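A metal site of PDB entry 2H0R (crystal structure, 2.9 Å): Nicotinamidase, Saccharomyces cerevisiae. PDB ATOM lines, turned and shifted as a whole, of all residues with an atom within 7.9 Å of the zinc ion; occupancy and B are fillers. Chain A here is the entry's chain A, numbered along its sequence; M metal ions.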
ATOM      1  N   ASP A   8       8.746   0.882  27.356  1.00  0.00           N
ATOM      2  CA  ASP A   8       8.457  -0.547  27.597  1.00  0.00           C
ATOM      3  C   ASP A   8       7.532  -0.908  28.777  1.00  0.00           C
ATOM      4  O   ASP A   8       7.758  -1.880  29.483  1.00  0.00           O
ATOM      5  CB  ASP A   8       9.780  -1.355  27.636  1.00  0.00           C
ATOM      6  CG  ASP A   8      10.562  -1.283  26.289  1.00  0.00           C
ATOM      7  OD1 ASP A   8      10.169  -0.499  25.382  1.00  0.00           O
ATOM      8  OD2 ASP A   8      11.558  -2.041  26.113  1.00  0.00           O
ATOM      9  N   GLN A  10       5.279  -2.879  29.350  1.00  0.00           N
ATOM     10  CA  GLN A  10       4.695  -4.066  28.751  1.00  0.00           C
ATOM     11  C   GLN A  10       4.503  -5.226  29.737  1.00  0.00           C
ATOM     12  O   GLN A  10       5.190  -5.336  30.780  1.00  0.00           O
ATOM     13  CB  GLN A  10       5.578  -4.520  27.614  1.00  0.00           C
ATOM     14  CG  GLN A  10       5.512  -3.639  26.357  1.00  0.00           C
ATOM     15  CD  GLN A  10       6.693  -3.871  25.438  1.00  0.00           C
ATOM     16  OE1 GLN A  10       7.819  -3.474  25.752  1.00  0.00           O
ATOM     17  NE2 GLN A  10       6.456  -4.537  24.314  1.00  0.00           N
ATOM     18  N   PHE A  13       7.365  -7.205  31.196  1.00  0.00           N
ATOM     19  CA  PHE A  13       8.200  -6.470  32.167  1.00  0.00           C
ATOM     20  C   PHE A  13       7.457  -6.049  33.438  1.00  0.00           C
ATOM     21  O   PHE A  13       8.074  -5.826  34.476  1.00  0.00           O
ATOM     22  CB  PHE A  13       8.779  -5.187  31.593  1.00  0.00           C
ATOM     23  CG  PHE A  13       9.702  -5.400  30.460  1.00  0.00           C
ATOM     24  CD1 PHE A  13      10.817  -6.211  30.604  1.00  0.00           C
ATOM     25  CD2 PHE A  13       9.484  -4.772  29.246  1.00  0.00           C
ATOM     26  CE1 PHE A  13      11.679  -6.403  29.536  1.00  0.00           C
ATOM     27  CE2 PHE A  13      10.339  -4.972  28.177  1.00  0.00           C
ATOM     28  CZ  PHE A  13      11.425  -5.784  28.324  1.00  0.00           C
ATOM     29  N   LEU A  20       9.809 -11.478  32.331  1.00  0.00           N
ATOM     30  CA  LEU A  20      10.983 -10.710  32.778  1.00  0.00           C
ATOM     31  C   LEU A  20      10.554  -9.581  33.705  1.00  0.00           C
ATOM     32  O   LEU A  20      10.950  -8.430  33.565  1.00  0.00           O
ATOM     33  CB  LEU A  20      11.676 -10.165  31.543  1.00  0.00           C
ATOM     34  CG  LEU A  20      13.152  -9.836  31.580  1.00  0.00           C
ATOM     35  CD1 LEU A  20      13.917 -10.897  32.363  1.00  0.00           C
ATOM     36  CD2 LEU A  20      13.576  -9.771  30.113  1.00  0.00           C
ATOM     37  N   ARG A  50       7.673  -0.030  22.558  1.00  0.00           N
ATOM     38  CA  ARG A  50       7.532  -1.445  22.908  1.00  0.00           C
ATOM     39  C   ARG A  50       8.782  -2.192  22.450  1.00  0.00           C
ATOM     40  O   ARG A  50       9.257  -1.941  21.342  1.00  0.00           O
ATOM     41  CB  ARG A  50       6.324  -2.026  22.184  1.00  0.00           C
ATOM     42  CG  ARG A  50       4.999  -1.506  22.689  1.00  0.00           C
ATOM     43  CD  ARG A  50       3.845  -2.186  21.995  1.00  0.00           C
ATOM     44  NE  ARG A  50       4.049  -2.056  20.567  1.00  0.00           N
ATOM     45  CZ  ARG A  50       3.177  -2.344  19.621  1.00  0.00           C
ATOM     46  NH1 ARG A  50       2.003  -2.800  19.909  1.00  0.00           N
ATOM     47  NH2 ARG A  50       3.541  -2.200  18.346  1.00  0.00           N
ATOM     48  N   ASP A  51       9.311  -3.072  23.291  1.00  0.00           N
ATOM     49  CA  ASP A  51      10.190  -4.133  22.810  1.00  0.00           C
ATOM     50  C   ASP A  51       9.284  -5.025  21.959  1.00  0.00           C
ATOM     51  O   ASP A  51       8.259  -5.512  22.435  1.00  0.00           O
ATOM     52  CB  ASP A  51      10.714  -4.949  23.984  1.00  0.00           C
ATOM     53  CG  ASP A  51      12.187  -5.238  23.897  1.00  0.00           C
ATOM     54  OD1 ASP A  51      12.891  -4.397  23.297  1.00  0.00           O
ATOM     55  OD2 ASP A  51      12.673  -6.274  24.428  1.00  0.00           O
ATOM     56  N   TRP A  52       9.666  -5.262  20.716  1.00  0.00           N
ATOM     57  CA  TRP A  52       8.814  -5.959  19.766  1.00  0.00           C
ATOM     58  C   TRP A  52       9.578  -7.079  19.025  1.00  0.00           C
ATOM     59  O   TRP A  52       9.823  -6.984  17.842  1.00  0.00           O
ATOM     60  CB  TRP A  52       8.319  -4.904  18.801  1.00  0.00           C
ATOM     61  CG  TRP A  52       7.093  -5.246  18.047  1.00  0.00           C
ATOM     62  CD1 TRP A  52       6.992  -5.414  16.714  1.00  0.00           C
ATOM     63  CD2 TRP A  52       5.782  -5.432  18.581  1.00  0.00           C
ATOM     64  NE1 TRP A  52       5.717  -5.712  16.367  1.00  0.00           N
ATOM     65  CE2 TRP A  52       4.938  -5.735  17.489  1.00  0.00           C
ATOM     66  CE3 TRP A  52       5.229  -5.392  19.865  1.00  0.00           C
ATOM     67  CZ2 TRP A  52       3.569  -6.009  17.658  1.00  0.00           C
ATOM     68  CZ3 TRP A  52       3.868  -5.646  20.022  1.00  0.00           C
ATOM     69  CH2 TRP A  52       3.063  -5.956  18.920  1.00  0.00           C
ATOM     70  N   HIS A  53       9.946  -8.155  19.700  1.00  0.00           N
ATOM     71  CA  HIS A  53      10.831  -9.189  19.122  1.00  0.00           C
ATOM     72  C   HIS A  53      10.160 -10.277  18.256  1.00  0.00           C
ATOM     73  O   HIS A  53       9.036 -10.709  18.542  1.00  0.00           O
ATOM     74  CB  HIS A  53      11.574  -9.913  20.253  1.00  0.00           C
ATOM     75  CG  HIS A  53      12.467  -9.035  21.071  1.00  0.00           C
ATOM     76  ND1 HIS A  53      13.474  -8.268  20.517  1.00  0.00           N
ATOM     77  CD2 HIS A  53      12.551  -8.853  22.408  1.00  0.00           C
ATOM     78  CE1 HIS A  53      14.101  -7.619  21.481  1.00  0.00           C
ATOM     79  NE2 HIS A  53      13.559  -7.959  22.638  1.00  0.00           N
ATOM     80  N   HIS A  57      14.495 -14.252  17.953  1.00  0.00           N
ATOM     81  CA  HIS A  57      15.404 -13.147  18.198  1.00  0.00           C
ATOM     82  C   HIS A  57      16.726 -13.557  18.842  1.00  0.00           C
ATOM     83  O   HIS A  57      16.765 -14.446  19.687  1.00  0.00           O
ATOM     84  CB  HIS A  57      14.727 -12.093  19.065  1.00  0.00           C
ATOM     85  CG  HIS A  57      15.419 -10.777  19.024  1.00  0.00           C
ATOM     86  ND1 HIS A  57      16.200 -10.314  20.066  1.00  0.00           N
ATOM     87  CD2 HIS A  57      15.500  -9.839  18.046  1.00  0.00           C
ATOM     88  CE1 HIS A  57      16.703  -9.138  19.739  1.00  0.00           C
ATOM     89  NE2 HIS A  57      16.294  -8.832  18.516  1.00  0.00           N
ATOM     90  N   SER A  59      18.485 -12.300  20.934  1.00  0.00           N
ATOM     91  CA  SER A  59      18.705 -11.868  22.298  1.00  0.00           C
ATOM     92  C   SER A  59      18.140 -12.833  23.295  1.00  0.00           C
ATOM     93  O   SER A  59      18.421 -12.676  24.457  1.00  0.00           O
ATOM     94  CB  SER A  59      18.243 -10.425  22.544  1.00  0.00           C
ATOM     95  OG  SER A  59      16.873 -10.275  22.876  1.00  0.00           O
ATOM     96  N   PHE A  60      17.379 -13.842  22.844  1.00  0.00           N
ATOM     97  CA  PHE A  60      16.810 -14.890  23.738  1.00  0.00           C
ATOM     98  C   PHE A  60      17.739 -16.093  23.885  1.00  0.00           C
ATOM     99  O   PHE A  60      18.192 -16.665  22.888  1.00  0.00           O
ATOM    100  CB  PHE A  60      15.506 -15.453  23.196  1.00  0.00           C
ATOM    101  CG  PHE A  60      14.476 -14.431  22.906  1.00  0.00           C
ATOM    102  CD1 PHE A  60      14.418 -13.235  23.624  1.00  0.00           C
ATOM    103  CD2 PHE A  60      13.520 -14.673  21.922  1.00  0.00           C
ATOM    104  CE1 PHE A  60      13.443 -12.273  23.347  1.00  0.00           C
ATOM    105  CE2 PHE A  60      12.557 -13.735  21.631  1.00  0.00           C
ATOM    106  CZ  PHE A  60      12.519 -12.515  22.350  1.00  0.00           C
ATOM    107  N   TRP A  91      18.581 -13.294  27.313  1.00  0.00           N
ATOM    108  CA  TRP A  91      17.431 -13.191  28.218  1.00  0.00           C
ATOM    109  C   TRP A  91      16.407 -14.324  28.105  1.00  0.00           C
ATOM    110  O   TRP A  91      16.364 -15.042  27.110  1.00  0.00           O
ATOM    111  CB  TRP A  91      16.684 -11.908  27.885  1.00  0.00           C
ATOM    112  CG  TRP A  91      17.468 -10.684  28.112  1.00  0.00           C
ATOM    113  CD1 TRP A  91      17.998  -9.889  27.184  1.00  0.00           C
ATOM    114  CD2 TRP A  91      17.783 -10.091  29.371  1.00  0.00           C
ATOM    115  NE1 TRP A  91      18.645  -8.831  27.756  1.00  0.00           N
ATOM    116  CE2 TRP A  91      18.528  -8.925  29.107  1.00  0.00           C
ATOM    117  CE3 TRP A  91      17.529 -10.448  30.707  1.00  0.00           C
ATOM    118  CZ2 TRP A  91      19.022  -8.102  30.125  1.00  0.00           C
ATOM    119  CZ3 TRP A  91      18.019  -9.635  31.715  1.00  0.00           C
ATOM    120  CH2 TRP A  91      18.750  -8.468  31.416  1.00  0.00           C
ATOM    121  N   PRO A  92      15.513 -14.452  29.079  1.00  0.00           N
ATOM    122  CA  PRO A  92      14.332 -15.265  28.836  1.00  0.00           C
ATOM    123  C   PRO A  92      13.527 -14.683  27.658  1.00  0.00           C
ATOM    124  O   PRO A  92      13.690 -13.522  27.322  1.00  0.00           O
ATOM    125  CB  PRO A  92      13.547 -15.083  30.112  1.00  0.00           C
ATOM    126  CG  PRO A  92      14.551 -14.765  31.106  1.00  0.00           C
ATOM    127  CD  PRO A  92      15.488 -13.893  30.435  1.00  0.00           C
ATOM    128  N   VAL A  93      12.691 -15.489  27.031  1.00  0.00           N
ATOM    129  CA  VAL A  93      11.962 -15.036  25.862  1.00  0.00           C
ATOM    130  C   VAL A  93      10.983 -13.956  26.326  1.00  0.00           C
ATOM    131  O   VAL A  93      10.210 -14.183  27.262  1.00  0.00           O
ATOM    132  CB  VAL A  93      11.166 -16.174  25.213  1.00  0.00           C
ATOM    133  CG1 VAL A  93      10.265 -15.621  24.110  1.00  0.00           C
ATOM    134  CG2 VAL A  93      12.093 -17.301  24.711  1.00  0.00           C
ATOM    135  N   HIS A  94      10.979 -12.796  25.708  1.00  0.00           N
ATOM    136  CA  HIS A  94      10.095 -11.758  26.223  1.00  0.00           C
ATOM    137  C   HIS A  94       9.624 -10.908  25.057  1.00  0.00           C
ATOM    138  O   HIS A  94      10.255 -10.909  24.016  1.00  0.00           O
ATOM    139  CB  HIS A  94      10.834 -10.919  27.248  1.00  0.00           C
ATOM    140  CG  HIS A  94      12.063 -10.287  26.708  1.00  0.00           C
ATOM    141  ND1 HIS A  94      13.288 -10.907  26.704  1.00  0.00           N
ATOM    142  CD2 HIS A  94      12.249  -9.078  26.099  1.00  0.00           C
ATOM    143  CE1 HIS A  94      14.179 -10.121  26.139  1.00  0.00           C
ATOM    144  NE2 HIS A  94      13.578  -9.009  25.754  1.00  0.00           N
ATOM    145  N   CYS A  95       8.513 -10.210  25.224  1.00  0.00           N
ATOM    146  CA  CYS A  95       7.998  -9.293  24.213  1.00  0.00           C
ATOM    147  C   CYS A  95       7.976  -9.794  22.753  1.00  0.00           C
ATOM    148  O   CYS A  95       8.343  -9.072  21.837  1.00  0.00           O
ATOM    149  CB  CYS A  95       8.731  -7.982  24.341  1.00  0.00           C
ATOM    150  SG  CYS A  95       8.652  -7.410  26.046  1.00  0.00           S
ATOM    151  N   LYS A 122      10.879  -1.305  19.065  1.00  0.00           N
ATOM    152  CA  LYS A 122      12.317  -1.574  18.935  1.00  0.00           C
ATOM    153  C   LYS A 122      12.529  -3.075  19.031  1.00  0.00           C
ATOM    154  O   LYS A 122      11.647  -3.787  19.525  1.00  0.00           O
ATOM    155  CB  LYS A 122      13.097  -0.838  20.017  1.00  0.00           C
ATOM    156  CG  LYS A 122      12.731  -1.262  21.419  1.00  0.00           C
ATOM    157  CD  LYS A 122      13.447  -0.415  22.416  1.00  0.00           C
ATOM    158  CE  LYS A 122      13.131  -0.831  23.850  1.00  0.00           C
ATOM    159  NZ  LYS A 122      14.070  -1.836  24.521  1.00  0.00           N
ATOM    160  N   GLY A 123      13.674  -3.579  18.604  1.00  0.00           N
ATOM    161  CA  GLY A 123      13.982  -4.998  18.847  1.00  0.00           C
ATOM    162  C   GLY A 123      13.438  -5.946  17.784  1.00  0.00           C
ATOM    163  O   GLY A 123      13.621  -7.158  17.818  1.00  0.00           O
ATOM    164  N   ARG A 128      19.858  -8.567  15.959  1.00  0.00           N
ATOM    165  CA  ARG A 128      20.538  -7.617  16.817  1.00  0.00           C
ATOM    166  C   ARG A 128      19.655  -7.205  18.002  1.00  0.00           C
ATOM    167  O   ARG A 128      18.417  -7.102  17.885  1.00  0.00           O
ATOM    168  CB  ARG A 128      20.912  -6.397  15.993  1.00  0.00           C
ATOM    169  CG  ARG A 128      19.710  -5.565  15.584  1.00  0.00           C
ATOM    170  CD  ARG A 128      19.963  -4.682  14.428  1.00  0.00           C
ATOM    171  NE  ARG A 128      20.307  -5.480  13.282  1.00  0.00           N
ATOM    172  CZ  ARG A 128      20.852  -5.001  12.177  1.00  0.00           C
ATOM    173  NH1 ARG A 128      21.105  -3.694  12.080  1.00  0.00           N
ATOM    174  NH2 ARG A 128      21.132  -5.845  11.168  1.00  0.00           N
ATOM    175  N   GLU A 129      20.307  -6.952  19.127  1.00  0.00           N
ATOM    176  CA  GLU A 129      19.655  -6.365  20.280  1.00  0.00           C
ATOM    177  C   GLU A 129      19.472  -4.856  20.054  1.00  0.00           C
ATOM    178  O   GLU A 129      20.305  -4.236  19.375  1.00  0.00           O
ATOM    179  CB  GLU A 129      20.522  -6.611  21.515  1.00  0.00           C
ATOM    180  CG  GLU A 129      20.021  -6.017  22.830  1.00  0.00           C
ATOM    181  CD  GLU A 129      18.682  -6.578  23.280  1.00  0.00           C
ATOM    182  OE1 GLU A 129      17.646  -6.189  22.700  1.00  0.00           O
ATOM    183  OE2 GLU A 129      18.669  -7.403  24.227  1.00  0.00           O
ATOM    184  N   TYR A 130      18.383  -4.288  20.590  1.00  0.00           N
ATOM    185  CA  TYR A 130      18.260  -2.850  20.765  1.00  0.00           C
ATOM    186  C   TYR A 130      17.893  -2.531  22.187  1.00  0.00           C
ATOM    187  O   TYR A 130      16.822  -2.898  22.622  1.00  0.00           O
ATOM    188  CB  TYR A 130      17.034  -2.246  20.125  1.00  0.00           C
ATOM    189  CG  TYR A 130      16.764  -2.319  18.693  1.00  0.00           C
ATOM    190  CD1 TYR A 130      16.725  -3.543  18.059  1.00  0.00           C
ATOM    191  CD2 TYR A 130      16.418  -1.168  17.981  1.00  0.00           C
ATOM    192  CE1 TYR A 130      16.399  -3.642  16.752  1.00  0.00           C
ATOM    193  CE2 TYR A 130      16.091  -1.240  16.669  1.00  0.00           C
ATOM    194  CZ  TYR A 130      16.077  -2.500  16.068  1.00  0.00           C
ATOM    195  OH  TYR A 130      15.747  -2.687  14.753  1.00  0.00           O
ATOM    196  N   TYR A 131      18.670  -1.731  22.884  1.00  0.00           N
ATOM    197  CA  TYR A 131      18.128  -1.216  24.128  1.00  0.00           C
ATOM    198  C   TYR A 131      17.454   0.129  23.919  1.00  0.00           C
ATOM    199  O   TYR A 131      16.330   0.339  24.387  1.00  0.00           O
ATOM    200  CB  TYR A 131      19.202  -1.207  25.177  1.00  0.00           C
ATOM    201  CG  TYR A 131      19.543  -2.601  25.644  1.00  0.00           C
ATOM    202  CD1 TYR A 131      18.524  -3.514  25.937  1.00  0.00           C
ATOM    203  CD2 TYR A 131      20.855  -3.002  25.795  1.00  0.00           C
ATOM    204  CE1 TYR A 131      18.807  -4.793  26.382  1.00  0.00           C
ATOM    205  CE2 TYR A 131      21.165  -4.279  26.247  1.00  0.00           C
ATOM    206  CZ  TYR A 131      20.120  -5.170  26.550  1.00  0.00           C
ATOM    207  OH  TYR A 131      20.416  -6.434  26.996  1.00  0.00           O
ATOM    208  N   CYS A 167      16.796  -0.262  28.922  1.00  0.00           N
ATOM    209  CA  CYS A 167      16.171   0.554  27.868  1.00  0.00           C
ATOM    210  C   CYS A 167      15.941   2.027  28.292  1.00  0.00           C
ATOM    211  O   CYS A 167      16.065   2.922  27.466  1.00  0.00           O
ATOM    212  CB  CYS A 167      14.898  -0.098  27.296  1.00  0.00           C
ATOM    213  SG  CYS A 167      14.748  -1.943  27.532  1.00  0.00           S
HETATM  214 ZN    ZN M   1      14.339  -7.395  24.445  1.00  0.00          ZN
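OD1 of Asp 8 lies within hydrogen-bond range of N of Asp 51 (3.4 Å). O of Cys 95 sits at hydrogen-bond distance from N of His 53, 2.8 Å away. A ring nitrogen (ND1) of His 53 lies within hydrogen-bond range of the backbone carbonyl oxygen (O) of Gly 123, 2.9 Å away. A ring nitrogen (ND1) of His 53 lies close to a ring nitrogen (ND1) of His 57 (3.4 Å). NZ of Lys 122 is in salt-bridge range of OD1 of Asp 51, 3.1 Å away. The side-chain hydroxyl of Tyr 131 sits close to the side-chain carboxylate of Glu 129 (3.4 Å). The side-chain amide nitrogen (NE2) of Gln 10 sits at hydrogen-bond distance from the backbone carbonyl oxygen (O) of Asp 51 (2.8 Å). A ring nitrogen (ND1) of His 94 lies within hydrogen-bond range of the backbone carbonyl oxygen of Pro 92, at 2.7 Å.
Residues that only touch the zinc ion: Glu 129 (3.9 Å). Four residues have an atom within 4 Å of the zinc ion: Asp 51, His 53, His 94 and Glu 129. The nearest printed residue that does not touch the zinc ion is Ser 59 (4.1 Å).
The side-chain carboxylate (OD2) of Asp 51 is bound to the zinc ion (2.0 Å). NE2 of His 53 binds the zinc ion (2.0 Å). The zinc ion is bound by NE2 of His 94, 2.2 Å away.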
